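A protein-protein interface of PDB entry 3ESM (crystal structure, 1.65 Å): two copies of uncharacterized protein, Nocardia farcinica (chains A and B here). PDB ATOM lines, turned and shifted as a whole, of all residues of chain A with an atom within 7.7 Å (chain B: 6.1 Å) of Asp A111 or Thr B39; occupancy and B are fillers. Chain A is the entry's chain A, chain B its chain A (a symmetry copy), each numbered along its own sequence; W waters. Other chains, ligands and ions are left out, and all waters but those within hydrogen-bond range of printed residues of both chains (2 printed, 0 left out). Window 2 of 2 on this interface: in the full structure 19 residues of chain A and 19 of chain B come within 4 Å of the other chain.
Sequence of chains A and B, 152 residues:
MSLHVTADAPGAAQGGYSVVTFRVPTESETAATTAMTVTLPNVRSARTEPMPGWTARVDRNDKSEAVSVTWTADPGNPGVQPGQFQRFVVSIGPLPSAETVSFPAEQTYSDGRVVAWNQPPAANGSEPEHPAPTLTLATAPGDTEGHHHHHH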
ATOM      1  N   SER A  28     -30.481  14.581   2.082  1.00  0.00           N
ATOM      2  CA  SER A  28     -30.719  15.153   3.376  1.00  0.00           C
ATOM      3  C   SER A  28     -31.679  16.290   3.136  1.00  0.00           C
ATOM      4  O   SER A  28     -31.708  16.879   2.051  1.00  0.00           O
ATOM      5  CB  SER A  28     -29.427  15.723   3.973  1.00  0.00           C
ATOM      6  OG  SER A  28     -29.719  16.483   5.126  1.00  0.00           O
ATOM      7  N   THR A  30     -31.419  18.960   5.117  1.00  0.00           N
ATOM      8  CA  THR A  30     -30.718  20.113   5.638  1.00  0.00           C
ATOM      9  C   THR A  30     -29.237  20.200   5.263  1.00  0.00           C
ATOM     10  O   THR A  30     -28.698  21.294   5.095  1.00  0.00           O
ATOM     11  CB  THR A  30     -30.798  20.134   7.153  1.00  0.00           C
ATOM     12  OG1 THR A  30     -30.461  18.826   7.657  1.00  0.00           O
ATOM     13  CG2 THR A  30     -32.229  20.507   7.570  1.00  0.00           C
ATOM     14  N   ALA A  31     -28.574  19.060   5.152  1.00  0.00           N
ATOM     15  CA  ALA A  31     -27.111  19.060   4.949  1.00  0.00           C
ATOM     16  C   ALA A  31     -26.795  18.954   3.451  1.00  0.00           C
ATOM     17  O   ALA A  31     -27.606  18.427   2.674  1.00  0.00           O
ATOM     18  CB  ALA A  31     -26.516  17.896   5.688  1.00  0.00           C
ATOM     19  N   ALA A  32     -25.617  19.451   3.050  1.00  0.00           N
ATOM     20  CA  ALA A  32     -25.246  19.516   1.634  1.00  0.00           C
ATOM     21  C   ALA A  32     -24.078  18.570   1.376  1.00  0.00           C
ATOM     22  O   ALA A  32     -23.341  18.257   2.304  1.00  0.00           O
ATOM     23  CB  ALA A  32     -24.821  20.937   1.301  1.00  0.00           C
ATOM     24  N   THR A  33     -23.928  18.095   0.148  1.00  0.00           N
ATOM     25  CA  THR A  33     -22.777  17.254  -0.166  1.00  0.00           C
ATOM     26  C   THR A  33     -21.556  18.168  -0.365  1.00  0.00           C
ATOM     27  O   THR A  33     -21.578  19.053  -1.234  1.00  0.00           O
ATOM     28  CB  THR A  33     -22.979  16.460  -1.450  1.00  0.00           C
ATOM     29  OG1 THR A  33     -24.085  15.566  -1.261  1.00  0.00           O
ATOM     30  CG2 THR A  33     -21.704  15.652  -1.771  1.00  0.00           C
ATOM     31  N   THR A  34     -20.498  17.879   0.389  1.00  0.00           N
ATOM     32  CA  THR A  34     -19.253  18.692   0.344  1.00  0.00           C
ATOM     33  C   THR A  34     -18.010  17.968  -0.147  1.00  0.00           C
ATOM     34  O   THR A  34     -16.997  18.608  -0.479  1.00  0.00           O
ATOM     35  CB  THR A  34     -18.931  19.306   1.708  1.00  0.00           C
ATOM     36  OG1 THR A  34     -18.750  18.253   2.674  1.00  0.00           O
ATOM     37  CG2 THR A  34     -20.081  20.244   2.122  1.00  0.00           C
ATOM     38  N   THR A 108     -19.506  12.816   1.542  1.00  0.00           N
ATOM     39  CA  THR A 108     -19.456  13.567   2.771  1.00  0.00           C
ATOM     40  C   THR A 108     -20.484  14.681   2.748  1.00  0.00           C
ATOM     41  O   THR A 108     -20.591  15.398   1.726  1.00  0.00           O
ATOM     42  CB  THR A 108     -18.054  14.224   2.949  1.00  0.00           C
ATOM     43  OG1 THR A 108     -17.032  13.208   3.073  1.00  0.00           O
ATOM     44  CG2 THR A 108     -18.043  15.112   4.172  1.00  0.00           C
ATOM     45  N   TYR A 109     -21.183  14.851   3.882  1.00  0.00           N
ATOM     46  CA  TYR A 109     -22.159  15.934   4.054  1.00  0.00           C
ATOM     47  C   TYR A 109     -21.651  17.002   4.985  1.00  0.00           C
ATOM     48  O   TYR A 109     -20.785  16.738   5.821  1.00  0.00           O
ATOM     49  CB  TYR A 109     -23.443  15.378   4.640  1.00  0.00           C
ATOM     50  CG  TYR A 109     -24.297  14.664   3.621  1.00  0.00           C
ATOM     51  CD1 TYR A 109     -25.383  15.306   3.043  1.00  0.00           C
ATOM     52  CD2 TYR A 109     -24.046  13.340   3.272  1.00  0.00           C
ATOM     53  CE1 TYR A 109     -26.193  14.667   2.157  1.00  0.00           C
ATOM     54  CE2 TYR A 109     -24.880  12.676   2.384  1.00  0.00           C
ATOM     55  CZ  TYR A 109     -25.952  13.355   1.829  1.00  0.00           C
ATOM     56  OH  TYR A 109     -26.808  12.747   0.923  1.00  0.00           O
ATOM     57  N   SER A 110     -22.194  18.209   4.821  1.00  0.00           N
ATOM     58  CA  SER A 110     -21.774  19.348   5.615  1.00  0.00           C
ATOM     59  C   SER A 110     -21.926  19.173   7.118  1.00  0.00           C
ATOM     60  O   SER A 110     -21.267  19.889   7.898  1.00  0.00           O
ATOM     61  CB  SER A 110     -22.570  20.554   5.177  1.00  0.00           C
ATOM     62  OG  SER A 110     -23.958  20.293   5.272  1.00  0.00           O
ATOM     63  N   ASP A 111     -22.827  18.291   7.535  1.00  0.00           N
ATOM     64  CA  ASP A 111     -23.040  18.051   8.984  1.00  0.00           C
ATOM     65  C   ASP A 111     -22.082  17.023   9.587  1.00  0.00           C
ATOM     66  O   ASP A 111     -22.226  16.620  10.769  1.00  0.00           O
ATOM     67  CB  ASP A 111     -24.495  17.635   9.263  1.00  0.00           C
ATOM     68  CG  ASP A 111     -24.871  16.329   8.608  1.00  0.00           C
ATOM     69  OD1 ASP A 111     -23.982  15.650   8.042  1.00  0.00           O
ATOM     70  OD2 ASP A 111     -26.095  15.988   8.635  1.00  0.00           O
ATOM     71  N   GLY A 112     -21.110  16.581   8.789  1.00  0.00           N
ATOM     72  CA  GLY A 112     -20.102  15.660   9.276  1.00  0.00           C
ATOM     73  C   GLY A 112     -20.348  14.196   8.935  1.00  0.00           C
ATOM     74  O   GLY A 112     -19.444  13.379   9.078  1.00  0.00           O
ATOM     75  N   ARG A 113     -21.567  13.855   8.533  1.00  0.00           N
ATOM     76  CA  ARG A 113     -21.882  12.468   8.159  1.00  0.00           C
ATOM     77  C   ARG A 113     -21.213  12.074   6.834  1.00  0.00           C
ATOM     78  O   ARG A 113     -21.040  12.907   5.956  1.00  0.00           O
ATOM     79  CB  ARG A 113     -23.404  12.271   8.043  1.00  0.00           C
ATOM     80  CG  ARG A 113     -24.156  12.553   9.350  1.00  0.00           C
ATOM     81  CD  ARG A 113     -25.684  12.245   9.190  1.00  0.00           C
ATOM     82  NE  ARG A 113     -26.375  13.219   8.333  1.00  0.00           N
ATOM     83  CZ  ARG A 113     -26.732  13.008   7.059  1.00  0.00           C
ATOM     84  NH1 ARG A 113     -26.493  11.843   6.456  1.00  0.00           N
ATOM     85  NH2 ARG A 113     -27.341  13.970   6.379  1.00  0.00           N
ATOM     86  N   VAL A 114     -20.866  10.797   6.704  1.00  0.00           N
ATOM     87  CA  VAL A 114     -20.339  10.278   5.444  1.00  0.00           C
ATOM     88  C   VAL A 114     -21.165   9.055   5.114  1.00  0.00           C
ATOM     89  O   VAL A 114     -21.285   8.142   5.982  1.00  0.00           O
ATOM     90  CB  VAL A 114     -18.839   9.924   5.530  1.00  0.00           C
ATOM     91  CG1 VAL A 114     -18.369   9.283   4.214  1.00  0.00           C
ATOM     92  CG2 VAL A 114     -17.981  11.177   5.860  1.00  0.00           C
ATOM     93  N   THR B  37     -12.725  14.664   8.480  1.00  0.00           N
ATOM     94  CA  THR B  37     -13.879  15.509   8.732  1.00  0.00           C
ATOM     95  C   THR B  37     -14.265  15.330  10.191  1.00  0.00           C
ATOM     96  O   THR B  37     -14.398  14.202  10.623  1.00  0.00           O
ATOM     97  CB  THR B  37     -15.059  15.119   7.802  1.00  0.00           C
ATOM     98  OG1 THR B  37     -14.768  15.636   6.470  1.00  0.00           O
ATOM     99  CG2 THR B  37     -16.342  15.764   8.276  1.00  0.00           C
ATOM    100  N   VAL B  38     -14.443  16.408  10.940  1.00  0.00           N
ATOM    101  CA  VAL B  38     -14.823  16.266  12.349  1.00  0.00           C
ATOM    102  C   VAL B  38     -16.111  16.994  12.592  1.00  0.00           C
ATOM    103  O   VAL B  38     -16.278  18.132  12.160  1.00  0.00           O
ATOM    104  CB  VAL B  38     -13.750  16.845  13.280  1.00  0.00           C
ATOM    105  CG1 VAL B  38     -14.224  16.777  14.741  1.00  0.00           C
ATOM    106  CG2 VAL B  38     -12.464  16.088  13.115  1.00  0.00           C
ATOM    107  N   THR B  39     -17.020  16.346  13.329  1.00  0.00           N
ATOM    108  CA  THR B  39     -18.321  16.938  13.629  1.00  0.00           C
ATOM    109  C   THR B  39     -18.167  17.800  14.872  1.00  0.00           C
ATOM    110  O   THR B  39     -17.641  17.327  15.888  1.00  0.00           O
ATOM    111  CB  THR B  39     -19.327  15.822  13.930  1.00  0.00           C
ATOM    112  OG1 THR B  39     -19.579  15.065  12.740  1.00  0.00           O
ATOM    113  CG2 THR B  39     -20.616  16.401  14.455  1.00  0.00           C
ATOM    114  N   LEU B  40     -18.588  19.077  14.791  1.00  0.00           N
ATOM    115  CA  LEU B  40     -18.391  20.034  15.880  1.00  0.00           C
ATOM    116  C   LEU B  40     -19.698  20.289  16.591  1.00  0.00           C
ATOM    117  O   LEU B  40     -20.761  20.141  16.020  1.00  0.00           O
ATOM    118  CB  LEU B  40     -17.859  21.391  15.387  1.00  0.00           C
ATOM    119  CG  LEU B  40     -16.516  21.301  14.648  1.00  0.00           C
ATOM    120  CD1 LEU B  40     -16.210  22.646  13.984  1.00  0.00           C
ATOM    121  CD2 LEU B  40     -15.414  20.935  15.636  1.00  0.00           C
ATOM    122  N   PRO B  41     -19.600  20.698  17.851  1.00  0.00           N
ATOM    123  CA  PRO B  41     -20.818  20.774  18.630  1.00  0.00           C
ATOM    124  C   PRO B  41     -21.522  22.142  18.406  1.00  0.00           C
ATOM    125  O   PRO B  41     -21.802  22.911  19.356  1.00  0.00           O
ATOM    126  CB  PRO B  41     -20.319  20.586  20.070  1.00  0.00           C
ATOM    127  CG  PRO B  41     -18.898  21.064  20.062  1.00  0.00           C
ATOM    128  CD  PRO B  41     -18.382  20.723  18.661  1.00  0.00           C
ATOM    129  N   ASP B  59     -17.954  24.131   7.908  1.00  0.00           N
ATOM    130  CA  ASP B  59     -19.345  24.235   7.441  1.00  0.00           C
ATOM    131  C   ASP B  59     -20.249  24.832   8.527  1.00  0.00           C
ATOM    132  O   ASP B  59     -20.022  24.616   9.710  1.00  0.00           O
ATOM    133  CB  ASP B  59     -19.882  22.885   7.011  1.00  0.00           C
ATOM    134  CG  ASP B  59     -19.400  22.512   5.597  1.00  0.00           C
ATOM    135  OD1 ASP B  59     -20.097  22.892   4.620  1.00  0.00           O
ATOM    136  OD2 ASP B  59     -18.323  21.906   5.481  1.00  0.00           O
ATOM    137  N   VAL B  67     -20.779  23.469  12.275  1.00  0.00           N
ATOM    138  CA  VAL B  67     -21.301  22.104  12.456  1.00  0.00           C
ATOM    139  C   VAL B  67     -20.264  21.023  12.148  1.00  0.00           C
ATOM    140  O   VAL B  67     -20.392  19.873  12.598  1.00  0.00           O
ATOM    141  CB  VAL B  67     -22.597  21.831  11.631  1.00  0.00           C
ATOM    142  CG1 VAL B  67     -23.736  22.733  12.095  1.00  0.00           C
ATOM    143  CG2 VAL B  67     -22.359  22.051  10.159  1.00  0.00           C
ATOM    144  N   SER B  68     -19.259  21.365  11.346  1.00  0.00           N
ATOM    145  CA  SER B  68     -18.187  20.415  11.081  1.00  0.00           C
ATOM    146  C   SER B  68     -17.004  21.143  10.453  1.00  0.00           C
ATOM    147  O   SER B  68     -17.125  22.308  10.045  1.00  0.00           O
ATOM    148  CB  SER B  68     -18.655  19.317  10.133  1.00  0.00           C
ATOM    149  OG  SER B  68     -18.728  19.790   8.790  1.00  0.00           O
ATOM    150  N   VAL B  69     -15.865  20.467  10.425  1.00  0.00           N
ATOM    151  CA  VAL B  69     -14.654  21.052   9.816  1.00  0.00           C
ATOM    152  C   VAL B  69     -14.023  19.928   9.036  1.00  0.00           C
ATOM    153  O   VAL B  69     -14.041  18.760   9.479  1.00  0.00           O
ATOM    154  CB  VAL B  69     -13.678  21.617  10.871  1.00  0.00           C
ATOM    155  CG1 VAL B  69     -13.400  20.603  12.009  1.00  0.00           C
ATOM    156  CG2 VAL B  69     -12.360  22.078  10.207  1.00  0.00           C
ATOM    157  N   SER B 102     -18.344  15.060  22.590  1.00  0.00           N
ATOM    158  CA  SER B 102     -17.659  14.161  21.649  1.00  0.00           C
ATOM    159  C   SER B 102     -17.582  14.837  20.291  1.00  0.00           C
ATOM    160  O   SER B 102     -18.410  15.693  19.975  1.00  0.00           O
ATOM    161  CB  SER B 102     -18.328  12.791  21.552  1.00  0.00           C
ATOM    162  OG  SER B 102     -18.163  12.145  22.844  1.00  0.00           O
ATOM    163  N   PHE B 103     -16.621  14.366  19.492  1.00  0.00           N
ATOM    164  CA  PHE B 103     -16.378  14.902  18.149  1.00  0.00           C
ATOM    165  C   PHE B 103     -16.299  13.752  17.158  1.00  0.00           C
ATOM    166  O   PHE B 103     -15.225  13.358  16.762  1.00  0.00           O
ATOM    167  CB  PHE B 103     -15.084  15.709  18.107  1.00  0.00           C
ATOM    168  CG  PHE B 103     -15.022  16.825  19.099  1.00  0.00           C
ATOM    169  CD1 PHE B 103     -15.463  18.102  18.772  1.00  0.00           C
ATOM    170  CD2 PHE B 103     -14.502  16.603  20.365  1.00  0.00           C
ATOM    171  CE1 PHE B 103     -15.387  19.161  19.700  1.00  0.00           C
ATOM    172  CE2 PHE B 103     -14.415  17.652  21.310  1.00  0.00           C
ATOM    173  CZ  PHE B 103     -14.868  18.933  20.975  1.00  0.00           C
ATOM    174  N   PRO B 104     -17.446  13.238  16.742  1.00  0.00           N
ATOM    175  CA  PRO B 104     -17.471  12.123  15.773  1.00  0.00           C
ATOM    176  C   PRO B 104     -16.621  12.539  14.555  1.00  0.00           C
ATOM    177  O   PRO B 104     -16.691  13.705  14.145  1.00  0.00           O
ATOM    178  CB  PRO B 104     -18.948  12.006  15.414  1.00  0.00           C
ATOM    179  CG  PRO B 104     -19.671  12.505  16.646  1.00  0.00           C
ATOM    180  CD  PRO B 104     -18.790  13.586  17.260  1.00  0.00           C
ATOM    181  N   ALA B 105     -15.813  11.629  14.015  1.00  0.00           N
ATOM    182  CA  ALA B 105     -14.923  12.013  12.902  1.00  0.00           C
ATOM    183  C   ALA B 105     -14.971  10.972  11.796  1.00  0.00           C
ATOM    184  O   ALA B 105     -15.357   9.814  12.029  1.00  0.00           O
ATOM    185  CB  ALA B 105     -13.532  12.192  13.387  1.00  0.00           C
HETATM  186  O   HOH W   1     -14.723  13.886   4.458  1.00  0.00           O
HETATM  187  O   HOH W   2     -17.786  13.319  11.336  1.00  0.00           O
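The side-chain hydroxyl of Ser B68 sits at hydrogen-bond distance from the backbone carbonyl oxygen of Ser A110, 2.7 Å away.
Hydrophobic or aromatic side chains of chain B that line the printed part of chain A: Val B67.
The backbone carbonyl oxygen (O) of Ala A32 is in hydrogen-bond range of the backbone NH (N) of Ser A110 (2.8 Å). N of Thr A34 sits at hydrogen-bond distance from O of Thr A108 (2.8 Å). The side-chain carboxylate of Asp A111 lies within salt-bridge range of the guanidinium group of Arg A113 (2.8 Å). The backbone NH of Leu B40 sits at hydrogen-bond distance from the backbone carbonyl oxygen of Val B67, at 2.9 Å. The backbone carbonyl oxygen (O) of Asp B59 lies within hydrogen-bond range of the backbone NH (N) of Val B67, 2.9 Å away. The backbone NH of Asp B59 is in hydrogen-bond range of the backbone carbonyl oxygen of Ser B68, at 2.9 Å.
Water W1 bridges the side-chain hydroxyl of Thr B37 (2.7 Å) and the side-chain hydroxyl of Thr A108 (2.8 Å). Water W2 lies within hydrogen-bond range of O of Gly A112, OG1 of Thr B39 and O of Pro B104.
Asp A111 touches just one residue of chain B: Thr B39 (3.6 Å). Of the printed residues of chain A, Thr B39 touches Asp A111 (3.6 Å) and Gly A112 (3.6 Å). Of the printed residues of chain A, Ser B68 touches Ser A110 (2.7 Å) and Gly A112 (3.9 Å). Of the printed residues of chain A, Thr B37 touches Gly A112. Of the printed residues of chain B, Gly A112 touches Thr B37, Thr B39 and Ser B68. Thr A108 touches none of the printed residues of chain B. Pro B41 touches none of the printed residues of chain A. The nearest residue of chain A that does not touch Thr B39 is Arg A113 (4.8 Å). The nearest printed residue of chain B that does not touch Gly A112 is Val B67 (5.1 Å).
Among the printed residues, merely in contact across the chains: Thr A34 with Asp B59, Ser A110 with Asp B59, Ser A110 with Val B67, Asp A111 with Thr B39, Gly A112 with Thr B37, Gly A112 with Thr B39 and Gly A112 with Ser B68.
No position is printed for both chains.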
